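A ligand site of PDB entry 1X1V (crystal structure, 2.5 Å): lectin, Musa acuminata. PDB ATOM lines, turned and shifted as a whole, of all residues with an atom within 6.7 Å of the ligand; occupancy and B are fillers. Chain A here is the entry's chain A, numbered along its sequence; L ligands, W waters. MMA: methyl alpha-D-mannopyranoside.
The side-chain carboxylate (OD1) of Asp 35 sits at hydrogen-bond distance from the side-chain hydroxyl (OH) of Tyr 83 (2.7 Å). N of Asp 38 is in hydrogen-bond range of O of Phe 32 (2.8 Å). The side-chain carboxylate (OD1) of Asp 38 is in hydrogen-bond range of the backbone NH (N) of Gly 34 (3.4 Å).
The side-chain carboxylate of Asp 38 sits at hydrogen-bond distance from an oxygen (O4) of the ligand, at 2.5 Å. An oxygen (O6) of the ligand is in hydrogen-bond range of the backbone carbonyl oxygen (O) of Val 36. The backbone NH (N) of Asp 35 is in hydrogen-bond range of an oxygen (O6) of the ligand, 3.4 Å away. An oxygen (O3) of the ligand is in hydrogen-bond range of the backbone NH of Gly 60, 2.9 Å away. An oxygen (O6) of the ligand is in hydrogen-bond range of the backbone NH (N) of Gly 34 (3.2 Å). N of Val 36 is in hydrogen-bond range of O6 of the ligand (2.9 Å).
Residues that only touch the ligand: Gly 59 (3.6 Å) and Tyr 83 (3.6 Å). Hydrophobic or aromatic side chains that line the ligand: Val 36. Seven residues have an atom within 4 Å of the ligand: Gly 34, Asp 35, Val 36, Asp 38, Gly 59, Gly 60 and Tyr 83.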
ATOM      1  N   PHE A  32     -18.824 -27.350  26.140  1.00  0.00           N
ATOM      2  CA  PHE A  32     -19.306 -26.343  25.205  1.00  0.00           C
ATOM      3  C   PHE A  32     -20.668 -26.819  24.675  1.00  0.00           C
ATOM      4  O   PHE A  32     -20.793 -27.947  24.193  1.00  0.00           O
ATOM      5  CB  PHE A  32     -18.327 -26.152  24.052  1.00  0.00           C
ATOM      6  CG  PHE A  32     -17.047 -25.460  24.432  1.00  0.00           C
ATOM      7  CD1 PHE A  32     -16.869 -24.101  24.180  1.00  0.00           C
ATOM      8  CD2 PHE A  32     -16.011 -26.163  25.025  1.00  0.00           C
ATOM      9  CE1 PHE A  32     -15.691 -23.462  24.537  1.00  0.00           C
ATOM     10  CE2 PHE A  32     -14.833 -25.524  25.382  1.00  0.00           C
ATOM     11  CZ  PHE A  32     -14.669 -24.182  25.142  1.00  0.00           C
ATOM     12  N   SER A  33     -21.680 -25.965  24.780  1.00  0.00           N
ATOM     13  CA  SER A  33     -22.997 -26.281  24.268  1.00  0.00           C
ATOM     14  C   SER A  33     -23.751 -25.049  23.816  1.00  0.00           C
ATOM     15  O   SER A  33     -23.567 -23.940  24.341  1.00  0.00           O
ATOM     16  CB  SER A  33     -23.829 -26.984  25.331  1.00  0.00           C
ATOM     17  OG  SER A  33     -24.267 -26.055  26.303  1.00  0.00           O
ATOM     18  N   GLY A  34     -24.606 -25.261  22.821  1.00  0.00           N
ATOM     19  CA  GLY A  34     -25.607 -24.286  22.414  1.00  0.00           C
ATOM     20  C   GLY A  34     -26.909 -25.018  22.564  1.00  0.00           C
ATOM     21  O   GLY A  34     -27.247 -25.417  23.678  1.00  0.00           O
ATOM     22  N   ASP A  35     -27.599 -25.245  21.456  1.00  0.00           N
ATOM     23  CA  ASP A  35     -28.790 -26.103  21.484  1.00  0.00           C
ATOM     24  C   ASP A  35     -28.390 -27.583  21.450  1.00  0.00           C
ATOM     25  O   ASP A  35     -29.207 -28.451  21.740  1.00  0.00           O
ATOM     26  CB  ASP A  35     -29.851 -25.727  20.403  1.00  0.00           C
ATOM     27  CG  ASP A  35     -29.292 -25.621  18.998  1.00  0.00           C
ATOM     28  OD1 ASP A  35     -28.274 -26.317  18.724  1.00  0.00           O
ATOM     29  OD2 ASP A  35     -29.808 -24.911  18.100  1.00  0.00           O
ATOM     30  N   VAL A  36     -27.129 -27.852  21.145  1.00  0.00           N
ATOM     31  CA  VAL A  36     -26.568 -29.201  21.234  1.00  0.00           C
ATOM     32  C   VAL A  36     -25.233 -29.153  21.987  1.00  0.00           C
ATOM     33  O   VAL A  36     -24.700 -28.066  22.222  1.00  0.00           O
ATOM     34  CB  VAL A  36     -26.458 -29.836  19.800  1.00  0.00           C
ATOM     35  CG1 VAL A  36     -25.094 -30.474  19.507  1.00  0.00           C
ATOM     36  CG2 VAL A  36     -27.601 -30.843  19.585  1.00  0.00           C
ATOM     37  N   VAL A  37     -24.718 -30.300  22.398  1.00  0.00           N
ATOM     38  CA  VAL A  37     -23.402 -30.355  23.026  1.00  0.00           C
ATOM     39  C   VAL A  37     -22.314 -30.369  21.947  1.00  0.00           C
ATOM     40  O   VAL A  37     -22.143 -31.348  21.236  1.00  0.00           O
ATOM     41  CB  VAL A  37     -23.245 -31.584  23.944  1.00  0.00           C
ATOM     42  CG1 VAL A  37     -21.910 -31.557  24.638  1.00  0.00           C
ATOM     43  CG2 VAL A  37     -24.370 -31.629  24.981  1.00  0.00           C
ATOM     44  N   ASP A  38     -21.578 -29.267  21.840  1.00  0.00           N
ATOM     45  CA  ASP A  38     -20.562 -29.149  20.796  1.00  0.00           C
ATOM     46  C   ASP A  38     -19.315 -29.912  21.180  1.00  0.00           C
ATOM     47  O   ASP A  38     -18.785 -30.664  20.360  1.00  0.00           O
ATOM     48  CB  ASP A  38     -20.238 -27.685  20.509  1.00  0.00           C
ATOM     49  CG  ASP A  38     -21.407 -26.929  19.902  1.00  0.00           C
ATOM     50  OD1 ASP A  38     -22.387 -26.723  20.645  1.00  0.00           O
ATOM     51  OD2 ASP A  38     -21.451 -26.537  18.710  1.00  0.00           O
ATOM     52  N   SER A  58     -15.411 -26.975  17.944  1.00  0.00           N
ATOM     53  CA  SER A  58     -15.580 -25.531  18.160  1.00  0.00           C
ATOM     54  C   SER A  58     -17.066 -25.168  18.189  1.00  0.00           C
ATOM     55  O   SER A  58     -17.753 -25.494  19.166  1.00  0.00           O
ATOM     56  CB  SER A  58     -14.835 -24.767  17.056  1.00  0.00           C
ATOM     57  OG  SER A  58     -13.485 -25.186  16.988  1.00  0.00           O
ATOM     58  N   GLY A  59     -17.703 -24.354  18.415  1.00  0.00           N
ATOM     59  CA  GLY A  59     -19.122 -24.293  18.761  1.00  0.00           C
ATOM     60  C   GLY A  59     -19.509 -24.089  20.210  1.00  0.00           C
ATOM     61  O   GLY A  59     -18.876 -24.609  21.114  1.00  0.00           O
ATOM     62  N   GLY A  60     -20.569 -23.312  20.436  1.00  0.00           N
ATOM     63  CA  GLY A  60     -21.200 -23.230  21.752  1.00  0.00           C
ATOM     64  C   GLY A  60     -20.551 -22.313  22.766  1.00  0.00           C
ATOM     65  O   GLY A  60     -19.552 -21.640  22.489  1.00  0.00           O
ATOM     66  N   THR A  61     -21.150 -22.302  23.950  1.00  0.00           N
ATOM     67  CA  THR A  61     -20.689 -21.543  25.098  1.00  0.00           C
ATOM     68  C   THR A  61     -20.070 -22.514  26.093  1.00  0.00           C
ATOM     69  O   THR A  61     -20.613 -23.592  26.303  1.00  0.00           O
ATOM     70  CB  THR A  61     -21.891 -20.821  25.739  1.00  0.00           C
ATOM     71  OG1 THR A  61     -22.476 -19.944  24.784  1.00  0.00           O
ATOM     72  CG2 THR A  61     -21.479 -19.897  26.877  1.00  0.00           C
ATOM     73  N   TYR A  83     -29.941 -34.313  15.434  1.00  0.00           N
ATOM     74  CA  TYR A  83     -29.882 -32.875  15.205  1.00  0.00           C
ATOM     75  C   TYR A  83     -29.466 -32.676  13.765  1.00  0.00           C
ATOM     76  O   TYR A  83     -28.276 -32.736  13.432  1.00  0.00           O
ATOM     77  CB  TYR A  83     -28.862 -32.236  16.159  1.00  0.00           C
ATOM     78  CG  TYR A  83     -28.778 -30.714  16.105  1.00  0.00           C
ATOM     79  CD1 TYR A  83     -29.846 -29.932  16.504  1.00  0.00           C
ATOM     80  CD2 TYR A  83     -27.609 -30.076  15.695  1.00  0.00           C
ATOM     81  CE1 TYR A  83     -29.782 -28.560  16.479  1.00  0.00           C
ATOM     82  CE2 TYR A  83     -27.525 -28.674  15.666  1.00  0.00           C
ATOM     83  CZ  TYR A  83     -28.623 -27.926  16.060  1.00  0.00           C
ATOM     84  OH  TYR A  83     -28.600 -26.550  16.061  1.00  0.00           O
ATOM     85  N   GLY A 105     -26.922 -27.937  26.899  1.00  0.00           N
ATOM     86  CA  GLY A 105     -27.599 -28.298  25.653  1.00  0.00           C
ATOM     87  C   GLY A 105     -29.108 -28.184  25.776  1.00  0.00           C
ATOM     88  O   GLY A 105     -29.654 -28.388  26.861  1.00  0.00           O
ATOM     89  N   ASP A 130     -18.116 -32.268  14.393  1.00  0.00           N
ATOM     90  CA  ASP A 130     -18.574 -30.901  14.592  1.00  0.00           C
ATOM     91  C   ASP A 130     -19.164 -30.771  16.012  1.00  0.00           C
ATOM     92  O   ASP A 130     -19.033 -29.729  16.648  1.00  0.00           O
ATOM     93  CB  ASP A 130     -19.621 -30.552  13.530  1.00  0.00           C
ATOM     94  CG  ASP A 130     -19.737 -29.068  13.283  1.00  0.00           C
ATOM     95  OD1 ASP A 130     -18.873 -28.488  12.584  1.00  0.00           O
ATOM     96  OD2 ASP A 130     -20.712 -28.399  13.693  1.00  0.00           O
ATOM     97  N   PHE A 131     -19.813 -31.843  16.479  1.00  0.00           N
ATOM     98  CA  PHE A 131     -20.444 -31.880  17.821  1.00  0.00           C
ATOM     99  C   PHE A 131     -20.019 -33.157  18.572  1.00  0.00           C
ATOM    100  O   PHE A 131     -19.311 -33.978  18.003  1.00  0.00           O
ATOM    101  CB  PHE A 131     -21.975 -31.858  17.688  1.00  0.00           C
ATOM    102  CG  PHE A 131     -22.489 -30.810  16.736  1.00  0.00           C
ATOM    103  CD1 PHE A 131     -23.286 -31.170  15.638  1.00  0.00           C
ATOM    104  CD2 PHE A 131     -22.202 -29.468  16.934  1.00  0.00           C
ATOM    105  CE1 PHE A 131     -23.774 -30.210  14.757  1.00  0.00           C
ATOM    106  CE2 PHE A 131     -22.693 -28.499  16.052  1.00  0.00           C
ATOM    107  CZ  PHE A 131     -23.481 -28.876  14.964  1.00  0.00           C
HETATM  108  C1  MMA L   1     -26.015 -22.706  18.223  1.00  0.00           C
HETATM  109  C2  MMA L   1     -24.940 -21.842  18.807  1.00  0.00           C
HETATM  110  C3  MMA L   1     -23.659 -22.467  18.302  1.00  0.00           C
HETATM  111  C4  MMA L   1     -23.659 -23.969  18.596  1.00  0.00           C
HETATM  112  C5  MMA L   1     -24.967 -24.684  18.190  1.00  0.00           C
HETATM  113  C6  MMA L   1     -24.954 -26.180  18.512  1.00  0.00           C
HETATM  114  C7  MMA L   1     -27.745 -23.055  16.516  1.00  0.00           C
HETATM  115  O1  MMA L   1     -26.770 -22.223  17.146  1.00  0.00           O
HETATM  116  O2  MMA L   1     -24.980 -21.958  20.211  1.00  0.00           O
HETATM  117  O3  MMA L   1     -22.570 -21.848  18.944  1.00  0.00           O
HETATM  118  O4  MMA L   1     -22.603 -24.533  17.867  1.00  0.00           O
HETATM  119  O5  MMA L   1     -26.122 -24.027  18.676  1.00  0.00           O
HETATM  120  O6  MMA L   1     -24.870 -26.439  19.906  1.00  0.00           O
HETATM  121  O   HOH W   1     -27.286 -21.126  21.597  1.00  0.00           O
